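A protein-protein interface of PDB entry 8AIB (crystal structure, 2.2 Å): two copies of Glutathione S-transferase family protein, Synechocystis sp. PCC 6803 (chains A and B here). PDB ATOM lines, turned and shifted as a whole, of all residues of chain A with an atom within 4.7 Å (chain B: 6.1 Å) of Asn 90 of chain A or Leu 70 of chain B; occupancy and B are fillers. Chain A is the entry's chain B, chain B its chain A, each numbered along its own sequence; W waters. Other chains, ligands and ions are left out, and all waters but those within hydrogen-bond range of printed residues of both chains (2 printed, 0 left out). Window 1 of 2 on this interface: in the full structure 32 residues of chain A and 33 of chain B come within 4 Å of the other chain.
Leu 70 of chain A touches Asn 90 of chain B, and with the chains exchanged Asn 90 of chain A touches Leu 70 of chain B.
Arg 86 of chain A touches its own counterpart, Arg 86 of chain B.
Leu 94 of chain B touches its own counterpart, Leu 94 of chain A.
Water W1 lies within hydrogen-bond range of the backbone carbonyl oxygen (O) of Ala 67 of chain B (2.8 Å), the side-chain amide nitrogen (ND2) of Asn 90 of chain A (2.8 Å) and the backbone NH (N) of Tyr 71 of chain B (3.3 Å).
Water W2 bridges OE1 of Glu 74 of chain B (2.8 Å) and ND2 of Asn 90 of chain A (3.2 Å).
The guanidinium group (NH2) of Arg 86 of chain A is in salt-bridge range of the side-chain carboxylate (OE2) of Glu 74 of chain B (2.7 Å).
Of the printed residues of chain B, Arg 86 of chain A touches Glu 74 and Arg 86.
Asn 90 of chain A touches just these residues of chain B: Ala 67 (3.9 Å) and Leu 70 (3.97 Å).
Of the printed residues of chain A, Glu 64 of chain B touches Gln 91 (3.4 Å) and Leu 94 (3.9 Å).
Of the printed residues of chain A, Ala 67 of chain B touches Asn 90 (3.9 Å), Gln 91 (3.6 Å) and Leu 94 (3.9 Å).
Printed residues of chain A within 4 Å of Leu 70 of chain B: Asn 90 (3.97 Å).
Printed residues of chain A within 4 Å of Asn 90 of chain B: Leu 70.
Of the 10 printed residues of chain A, 6 touch a printed residue of chain B.
Printed residues of chain A that touch a printed residue of chain B: Leu 70, Arg 86, Ala 87, Asn 90, Gln 91 and Leu 94.
Of the 19 printed residues of chain B, 8 touch a printed residue of chain A.
Hydrophobic or aromatic side chains of chain B within 4 Å of the printed part of chain A: Ala 67, Leu 70, Tyr 71 and Leu 94.
Among the printed residues, 11 pairs touch across the chains.
CD1 of Leu 70 of chain A touches ND2 of Asn 90 of chain B, at 3.8 Å.
Arg 86 of chain A touches Arg 86 of chain B (NE to NE, 3.6 Å).
Ala 87 of chain A touches Tyr 71 of chain B (CB to CD1, 3.9 Å).
Asn 90 of chain A touches Ala 67 of chain B (C to CB, 3.9 Å).
CD1 of Leu 70 of chain B touches ND2 of Asn 90 of chain A (3.97 Å).
Gln 91 of chain A touches Glu 64 of chain B.
Ala 67 of chain B touches Gln 91 of chain A.
CB of Leu 94 of chain A touches CB of Glu 64 of chain B, 3.9 Å away.
Ala 67 of chain B touches Leu 94 of chain A (N to CG, 3.9 Å).
CD2 of Leu 94 of chain B touches CD2 of Leu 94 of chain A (3.6 Å).
OD1 of Asn 90 of chain B lies close to O of Arg 86 of chain B (3.0 Å).
NE2 of Gln 91 of chain A lies close to NE1 of Trp 92 of chain A (3.4 Å).
The backbone carbonyl oxygen (O) of Arg 86 of chain A sits close to the side-chain amide oxygen (OD1) of Asn 90 of chain A.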
ATOM      1  N   LEU A  70      34.685  -6.887   4.932  1.00  0.00           N
ATOM      2  CA  LEU A  70      34.217  -7.911   3.985  1.00  0.00           C
ATOM      3  C   LEU A  70      33.753  -7.275   2.684  1.00  0.00           C
ATOM      4  O   LEU A  70      34.036  -7.802   1.607  1.00  0.00           O
ATOM      5  CB  LEU A  70      33.094  -8.786   4.573  1.00  0.00           C
ATOM      6  CG  LEU A  70      33.437  -9.464   5.903  1.00  0.00           C
ATOM      7  CD1 LEU A  70      32.181  -9.910   6.657  1.00  0.00           C
ATOM      8  CD2 LEU A  70      34.402 -10.612   5.692  1.00  0.00           C
ATOM      9  N   ARG A  86      33.670 -17.306   0.946  1.00  0.00           N
ATOM     10  CA  ARG A  86      33.227 -16.102   1.658  1.00  0.00           C
ATOM     11  C   ARG A  86      32.951 -16.452   3.127  1.00  0.00           C
ATOM     12  O   ARG A  86      33.337 -15.693   3.989  1.00  0.00           O
ATOM     13  CB  ARG A  86      31.950 -15.546   1.044  1.00  0.00           C
ATOM     14  CG  ARG A  86      32.201 -14.554  -0.068  1.00  0.00           C
ATOM     15  CD  ARG A  86      30.912 -13.848  -0.443  1.00  0.00           C
ATOM     16  NE  ARG A  86      29.947 -14.798  -0.990  1.00  0.00           N
ATOM     17  CZ  ARG A  86      29.841 -15.097  -2.279  1.00  0.00           C
ATOM     18  NH1 ARG A  86      30.605 -14.479  -3.177  1.00  0.00           N
ATOM     19  NH2 ARG A  86      28.952 -15.989  -2.685  1.00  0.00           N
ATOM     20  N   ALA A  87      32.344 -17.618   3.409  1.00  0.00           N
ATOM     21  CA  ALA A  87      32.063 -18.089   4.770  1.00  0.00           C
ATOM     22  C   ALA A  87      33.315 -18.218   5.631  1.00  0.00           C
ATOM     23  O   ALA A  87      33.265 -17.850   6.788  1.00  0.00           O
ATOM     24  CB  ALA A  87      31.319 -19.418   4.733  1.00  0.00           C
ATOM     25  N   LEU A  88      34.443 -18.730   5.084  1.00  0.00           N
ATOM     26  CA  LEU A  88      35.678 -18.852   5.875  1.00  0.00           C
ATOM     27  C   LEU A  88      36.248 -17.469   6.201  1.00  0.00           C
ATOM     28  O   LEU A  88      36.800 -17.288   7.279  1.00  0.00           O
ATOM     29  CB  LEU A  88      36.724 -19.744   5.173  1.00  0.00           C
ATOM     30  CG  LEU A  88      36.264 -21.212   4.999  1.00  0.00           C
ATOM     31  CD1 LEU A  88      37.217 -22.003   4.091  1.00  0.00           C
ATOM     32  CD2 LEU A  88      36.085 -21.901   6.361  1.00  0.00           C
ATOM     33  N   VAL A  89      36.097 -16.489   5.288  1.00  0.00           N
ATOM     34  CA  VAL A  89      36.513 -15.125   5.586  1.00  0.00           C
ATOM     35  C   VAL A  89      35.531 -14.518   6.623  1.00  0.00           C
ATOM     36  O   VAL A  89      35.983 -14.008   7.635  1.00  0.00           O
ATOM     37  CB  VAL A  89      36.631 -14.264   4.308  1.00  0.00           C
ATOM     38  CG1 VAL A  89      36.910 -12.816   4.678  1.00  0.00           C
ATOM     39  CG2 VAL A  89      37.738 -14.803   3.385  1.00  0.00           C
ATOM     40  N   ASN A  90      34.210 -14.656   6.426  1.00  0.00           N
ATOM     41  CA  ASN A  90      33.195 -14.183   7.383  1.00  0.00           C
ATOM     42  C   ASN A  90      33.403 -14.791   8.801  1.00  0.00           C
ATOM     43  O   ASN A  90      33.254 -14.090   9.805  1.00  0.00           O
ATOM     44  CB  ASN A  90      31.789 -14.533   6.905  1.00  0.00           C
ATOM     45  CG  ASN A  90      31.345 -13.896   5.603  1.00  0.00           C
ATOM     46  OD1 ASN A  90      31.994 -13.000   5.066  1.00  0.00           O
ATOM     47  ND2 ASN A  90      30.209 -14.366   5.049  1.00  0.00           N
ATOM     48  N   GLN A  91      33.784 -16.081   8.886  1.00  0.00           N
ATOM     49  CA  GLN A  91      34.038 -16.768  10.164  1.00  0.00           C
ATOM     50  C   GLN A  91      35.064 -16.008  10.989  1.00  0.00           C
ATOM     51  O   GLN A  91      34.784 -15.676  12.138  1.00  0.00           O
ATOM     52  CB  GLN A  91      34.500 -18.235   9.906  1.00  0.00           C
ATOM     53  CG  GLN A  91      35.248 -18.934  11.043  1.00  0.00           C
ATOM     54  CD  GLN A  91      35.810 -20.250  10.531  1.00  0.00           C
ATOM     55  OE1 GLN A  91      35.100 -21.264  10.446  1.00  0.00           O
ATOM     56  NE2 GLN A  91      37.084 -20.256  10.165  1.00  0.00           N
ATOM     57  N   TRP A  92      36.201 -15.634  10.363  1.00  0.00           N
ATOM     58  CA  TRP A  92      37.272 -14.922  11.050  1.00  0.00           C
ATOM     59  C   TRP A  92      36.928 -13.467  11.410  1.00  0.00           C
ATOM     60  O   TRP A  92      37.391 -12.969  12.427  1.00  0.00           O
ATOM     61  CB  TRP A  92      38.558 -14.999  10.231  1.00  0.00           C
ATOM     62  CG  TRP A  92      39.166 -16.373  10.218  1.00  0.00           C
ATOM     63  CD1 TRP A  92      39.141 -17.279   9.197  1.00  0.00           C
ATOM     64  CD2 TRP A  92      39.899 -16.990  11.287  1.00  0.00           C
ATOM     65  NE1 TRP A  92      39.823 -18.418   9.562  1.00  0.00           N
ATOM     66  CE2 TRP A  92      40.299 -18.266  10.841  1.00  0.00           C
ATOM     67  CE3 TRP A  92      40.230 -16.596  12.589  1.00  0.00           C
ATOM     68  CZ2 TRP A  92      40.999 -19.158  11.657  1.00  0.00           C
ATOM     69  CZ3 TRP A  92      40.971 -17.461  13.377  1.00  0.00           C
ATOM     70  CH2 TRP A  92      41.339 -18.732  12.912  1.00  0.00           C
ATOM     71  N   ILE A  93      36.123 -12.795  10.589  1.00  0.00           N
ATOM     72  CA  ILE A  93      35.696 -11.419  10.865  1.00  0.00           C
ATOM     73  C   ILE A  93      34.723 -11.456  12.056  1.00  0.00           C
ATOM     74  O   ILE A  93      34.858 -10.647  12.950  1.00  0.00           O
ATOM     75  CB  ILE A  93      35.107 -10.707   9.588  1.00  0.00           C
ATOM     76  CG1 ILE A  93      36.225 -10.066   8.727  1.00  0.00           C
ATOM     77  CG2 ILE A  93      34.135  -9.583   9.984  1.00  0.00           C
ATOM     78  CD1 ILE A  93      37.240 -10.967   8.118  1.00  0.00           C
ATOM     79  N   LEU A  94      33.794 -12.433  12.099  1.00  0.00           N
ATOM     80  CA  LEU A  94      32.879 -12.596  13.234  1.00  0.00           C
ATOM     81  C   LEU A  94      33.670 -12.904  14.505  1.00  0.00           C
ATOM     82  O   LEU A  94      33.404 -12.337  15.559  1.00  0.00           O
ATOM     83  CB  LEU A  94      31.848 -13.706  12.981  1.00  0.00           C
ATOM     84  CG  LEU A  94      30.479 -13.223  12.473  1.00  0.00           C
ATOM     85  CD1 LEU A  94      29.853 -12.187  13.445  1.00  0.00           C
ATOM     86  CD2 LEU A  94      30.592 -12.608  11.103  1.00  0.00           C
ATOM     87  N   GLU B  64      31.361 -19.983  14.277  1.00  0.00           N
ATOM     88  CA  GLU B  64      30.823 -18.638  14.519  1.00  0.00           C
ATOM     89  C   GLU B  64      29.395 -18.658  14.026  1.00  0.00           C
ATOM     90  O   GLU B  64      29.166 -18.776  12.816  1.00  0.00           O
ATOM     91  CB  GLU B  64      31.618 -17.475  13.882  1.00  0.00           C
ATOM     92  CG  GLU B  64      32.913 -17.117  14.599  1.00  0.00           C
ATOM     93  CD  GLU B  64      32.715 -16.622  16.017  1.00  0.00           C
ATOM     94  OE1 GLU B  64      31.704 -15.926  16.275  1.00  0.00           O
ATOM     95  OE2 GLU B  64      33.584 -16.916  16.869  1.00  0.00           O
ATOM     96  N   SER B  65      28.428 -18.521  14.966  1.00  0.00           N
ATOM     97  CA  SER B  65      27.003 -18.532  14.683  1.00  0.00           C
ATOM     98  C   SER B  65      26.618 -17.534  13.590  1.00  0.00           C
ATOM     99  O   SER B  65      25.804 -17.862  12.721  1.00  0.00           O
ATOM    100  CB  SER B  65      26.198 -18.279  15.956  1.00  0.00           C
ATOM    101  OG  SER B  65      26.450 -16.997  16.512  1.00  0.00           O
ATOM    102  N   GLY B  66      27.249 -16.359  13.597  1.00  0.00           N
ATOM    103  CA  GLY B  66      26.968 -15.348  12.592  1.00  0.00           C
ATOM    104  C   GLY B  66      27.371 -15.784  11.194  1.00  0.00           C
ATOM    105  O   GLY B  66      26.596 -15.630  10.256  1.00  0.00           O
ATOM    106  N   ALA B  67      28.573 -16.353  11.040  1.00  0.00           N
ATOM    107  CA  ALA B  67      29.040 -16.807   9.729  1.00  0.00           C
ATOM    108  C   ALA B  67      28.178 -17.968   9.235  1.00  0.00           C
ATOM    109  O   ALA B  67      27.809 -18.008   8.049  1.00  0.00           O
ATOM    110  CB  ALA B  67      30.495 -17.237   9.811  1.00  0.00           C
ATOM    111  N   ILE B  68      27.778 -18.867  10.150  1.00  0.00           N
ATOM    112  CA  ILE B  68      26.884 -19.976   9.792  1.00  0.00           C
ATOM    113  C   ILE B  68      25.549 -19.442   9.286  1.00  0.00           C
ATOM    114  O   ILE B  68      25.030 -19.946   8.305  1.00  0.00           O
ATOM    115  CB  ILE B  68      26.658 -20.950  10.976  1.00  0.00           C
ATOM    116  CG1 ILE B  68      27.984 -21.546  11.504  1.00  0.00           C
ATOM    117  CG2 ILE B  68      25.675 -22.049  10.560  1.00  0.00           C
ATOM    118  CD1 ILE B  68      27.801 -22.309  12.769  1.00  0.00           C
ATOM    119  N   LEU B  69      24.983 -18.424   9.960  1.00  0.00           N
ATOM    120  CA  LEU B  69      23.712 -17.831   9.525  1.00  0.00           C
ATOM    121  C   LEU B  69      23.860 -17.233   8.110  1.00  0.00           C
ATOM    122  O   LEU B  69      23.027 -17.501   7.257  1.00  0.00           O
ATOM    123  CB  LEU B  69      23.258 -16.736  10.518  1.00  0.00           C
ATOM    124  CG  LEU B  69      22.640 -17.198  11.839  1.00  0.00           C
ATOM    125  CD1 LEU B  69      22.178 -15.998  12.662  1.00  0.00           C
ATOM    126  CD2 LEU B  69      21.440 -18.114  11.607  1.00  0.00           C
ATOM    127  N   LEU B  70      24.951 -16.487   7.852  1.00  0.00           N
ATOM    128  CA  LEU B  70      25.227 -15.896   6.527  1.00  0.00           C
ATOM    129  C   LEU B  70      25.402 -16.965   5.422  1.00  0.00           C
ATOM    130  O   LEU B  70      24.832 -16.833   4.330  1.00  0.00           O
ATOM    131  CB  LEU B  70      26.461 -14.983   6.583  1.00  0.00           C
ATOM    132  CG  LEU B  70      26.263 -13.723   7.416  1.00  0.00           C
ATOM    133  CD1 LEU B  70      27.587 -13.017   7.701  1.00  0.00           C
ATOM    134  CD2 LEU B  70      25.292 -12.794   6.738  1.00  0.00           C
ATOM    135  N   TYR B  71      26.151 -18.036   5.724  1.00  0.00           N
ATOM    136  CA  TYR B  71      26.361 -19.162   4.802  1.00  0.00           C
ATOM    137  C   TYR B  71      25.045 -19.858   4.465  1.00  0.00           C
ATOM    138  O   TYR B  71      24.786 -20.127   3.290  1.00  0.00           O
ATOM    139  CB  TYR B  71      27.344 -20.184   5.404  1.00  0.00           C
ATOM    140  CG  TYR B  71      27.496 -21.444   4.575  1.00  0.00           C
ATOM    141  CD1 TYR B  71      28.246 -21.443   3.412  1.00  0.00           C
ATOM    142  CD2 TYR B  71      26.888 -22.636   4.961  1.00  0.00           C
ATOM    143  CE1 TYR B  71      28.430 -22.603   2.672  1.00  0.00           C
ATOM    144  CE2 TYR B  71      27.040 -23.800   4.212  1.00  0.00           C
ATOM    145  CZ  TYR B  71      27.816 -23.776   3.065  1.00  0.00           C
ATOM    146  OH  TYR B  71      27.993 -24.895   2.292  1.00  0.00           O
ATOM    147  N   LEU B  72      24.226 -20.168   5.474  1.00  0.00           N
ATOM    148  CA  LEU B  72      22.941 -20.834   5.233  1.00  0.00           C
ATOM    149  C   LEU B  72      22.028 -19.940   4.365  1.00  0.00           C
ATOM    150  O   LEU B  72      21.381 -20.455   3.454  1.00  0.00           O
ATOM    151  CB  LEU B  72      22.222 -21.188   6.541  1.00  0.00           C
ATOM    152  CG  LEU B  72      22.893 -22.234   7.436  1.00  0.00           C
ATOM    153  CD1 LEU B  72      22.118 -22.400   8.734  1.00  0.00           C
ATOM    154  CD2 LEU B  72      23.059 -23.582   6.697  1.00  0.00           C
ATOM    155  N   ALA B  73      22.020 -18.607   4.627  1.00  0.00           N
ATOM    156  CA  ALA B  73      21.194 -17.662   3.877  1.00  0.00           C
ATOM    157  C   ALA B  73      21.630 -17.577   2.432  1.00  0.00           C
ATOM    158  O   ALA B  73      20.782 -17.478   1.552  1.00  0.00           O
ATOM    159  CB  ALA B  73      21.229 -16.271   4.524  1.00  0.00           C
ATOM    160  N   GLU B  74      22.945 -17.618   2.185  1.00  0.00           N
ATOM    161  CA  GLU B  74      23.486 -17.572   0.832  1.00  0.00           C
ATOM    162  C   GLU B  74      23.113 -18.847   0.101  1.00  0.00           C
ATOM    163  O   GLU B  74      22.618 -18.783  -1.018  1.00  0.00           O
ATOM    164  CB  GLU B  74      25.016 -17.465   0.868  1.00  0.00           C
ATOM    165  CG  GLU B  74      25.574 -16.065   0.972  1.00  0.00           C
ATOM    166  CD  GLU B  74      27.005 -16.041   0.472  1.00  0.00           C
ATOM    167  OE1 GLU B  74      27.896 -15.621   1.242  1.00  0.00           O
ATOM    168  OE2 GLU B  74      27.237 -16.463  -0.684  1.00  0.00           O
ATOM    169  N   LYS B  75      23.330 -20.007   0.742  1.00  0.00           N
ATOM    170  CA  LYS B  75      23.047 -21.327   0.184  1.00  0.00           C
ATOM    171  C   LYS B  75      21.564 -21.471  -0.201  1.00  0.00           C
ATOM    172  O   LYS B  75      21.256 -22.034  -1.244  1.00  0.00           O
ATOM    173  CB  LYS B  75      23.447 -22.403   1.210  1.00  0.00           C
ATOM    174  CG  LYS B  75      23.742 -23.762   0.616  1.00  0.00           C
ATOM    175  CD  LYS B  75      23.730 -24.868   1.695  1.00  0.00           C
ATOM    176  CE  LYS B  75      23.954 -26.235   1.077  1.00  0.00           C
ATOM    177  NZ  LYS B  75      24.012 -27.306   2.108  1.00  0.00           N
ATOM    178  N   ILE B  79      19.422 -14.083  -0.292  1.00  0.00           N
ATOM    179  CA  ILE B  79      20.071 -12.778  -0.418  1.00  0.00           C
ATOM    180  C   ILE B  79      20.388 -12.553  -1.889  1.00  0.00           C
ATOM    181  O   ILE B  79      20.935 -13.460  -2.519  1.00  0.00           O
ATOM    182  CB  ILE B  79      21.395 -12.752   0.405  1.00  0.00           C
ATOM    183  CG1 ILE B  79      21.182 -13.224   1.852  1.00  0.00           C
ATOM    184  CG2 ILE B  79      22.057 -11.376   0.350  1.00  0.00           C
ATOM    185  CD1 ILE B  79      22.442 -13.393   2.616  1.00  0.00           C
ATOM    186  N   ARG B  86      24.749  -8.495   0.144  1.00  0.00           N
ATOM    187  CA  ARG B  86      25.351  -9.351   1.160  1.00  0.00           C
ATOM    188  C   ARG B  86      25.905  -8.479   2.292  1.00  0.00           C
ATOM    189  O   ARG B  86      25.758  -8.833   3.450  1.00  0.00           O
ATOM    190  CB  ARG B  86      26.494 -10.176   0.562  1.00  0.00           C
ATOM    191  CG  ARG B  86      26.013 -11.413  -0.177  1.00  0.00           C
ATOM    192  CD  ARG B  86      27.179 -12.322  -0.494  1.00  0.00           C
ATOM    193  NE  ARG B  86      28.086 -11.697  -1.449  1.00  0.00           N
ATOM    194  CZ  ARG B  86      27.995 -11.841  -2.768  1.00  0.00           C
ATOM    195  NH1 ARG B  86      27.048 -12.606  -3.296  1.00  0.00           N
ATOM    196  NH2 ARG B  86      28.860 -11.234  -3.567  1.00  0.00           N
ATOM    197  N   VAL B  89      23.260  -7.631   4.935  1.00  0.00           N
ATOM    198  CA  VAL B  89      22.925  -8.710   5.845  1.00  0.00           C
ATOM    199  C   VAL B  89      24.101  -8.920   6.820  1.00  0.00           C
ATOM    200  O   VAL B  89      23.881  -9.030   8.022  1.00  0.00           O
ATOM    201  CB  VAL B  89      22.516  -9.998   5.096  1.00  0.00           C
ATOM    202  CG1 VAL B  89      22.194 -11.092   6.083  1.00  0.00           C
ATOM    203  CG2 VAL B  89      21.315  -9.740   4.178  1.00  0.00           C
ATOM    204  N   ASN B  90      25.347  -8.895   6.305  1.00  0.00           N
ATOM    205  CA  ASN B  90      26.577  -9.000   7.093  1.00  0.00           C
ATOM    206  C   ASN B  90      26.594  -7.934   8.220  1.00  0.00           C
ATOM    207  O   ASN B  90      26.941  -8.219   9.379  1.00  0.00           O
ATOM    208  CB  ASN B  90      27.806  -8.767   6.198  1.00  0.00           C
ATOM    209  CG  ASN B  90      28.077  -9.822   5.143  1.00  0.00           C
ATOM    210  OD1 ASN B  90      27.351 -10.827   5.009  1.00  0.00           O
ATOM    211  ND2 ASN B  90      29.137  -9.607   4.351  1.00  0.00           N
ATOM    212  N   ILE B  93      24.304  -8.992  10.999  1.00  0.00           N
ATOM    213  CA  ILE B  93      24.775 -10.169  11.720  1.00  0.00           C
ATOM    214  C   ILE B  93      25.928  -9.732  12.641  1.00  0.00           C
ATOM    215  O   ILE B  93      25.968 -10.119  13.806  1.00  0.00           O
ATOM    216  CB  ILE B  93      25.137 -11.334  10.719  1.00  0.00           C
ATOM    217  CG1 ILE B  93      23.914 -12.256  10.410  1.00  0.00           C
ATOM    218  CG2 ILE B  93      26.299 -12.184  11.222  1.00  0.00           C
ATOM    219  CD1 ILE B  93      22.671 -11.629  10.032  1.00  0.00           C
ATOM    220  N   LEU B  94      26.844  -8.894  12.135  1.00  0.00           N
ATOM    221  CA  LEU B  94      27.954  -8.367  12.962  1.00  0.00           C
ATOM    222  C   LEU B  94      27.400  -7.529  14.112  1.00  0.00           C
ATOM    223  O   LEU B  94      27.889  -7.598  15.242  1.00  0.00           O
ATOM    224  CB  LEU B  94      28.891  -7.490  12.124  1.00  0.00           C
ATOM    225  CG  LEU B  94      30.191  -8.138  11.602  1.00  0.00           C
ATOM    226  CD1 LEU B  94      31.021  -8.741  12.708  1.00  0.00           C
ATOM    227  CD2 LEU B  94      29.920  -9.113  10.538  1.00  0.00           C
ATOM    228  N   VAL B 138      17.040 -13.775   7.680  1.00  0.00           N
ATOM    229  CA  VAL B 138      18.090 -14.200   8.611  1.00  0.00           C
ATOM    230  C   VAL B 138      18.481 -13.064   9.590  1.00  0.00           C
ATOM    231  O   VAL B 138      18.925 -13.338  10.713  1.00  0.00           O
ATOM    232  CB  VAL B 138      19.311 -14.743   7.828  1.00  0.00           C
ATOM    233  CG1 VAL B 138      20.023 -13.628   7.072  1.00  0.00           C
ATOM    234  CG2 VAL B 138      20.273 -15.498   8.741  1.00  0.00           C
HETATM  235  O   HOH W   1      29.263 -16.852   5.970  1.00  0.00           O
HETATM  236  O   HOH W   2      28.351 -13.265   2.700  1.00  0.00           O
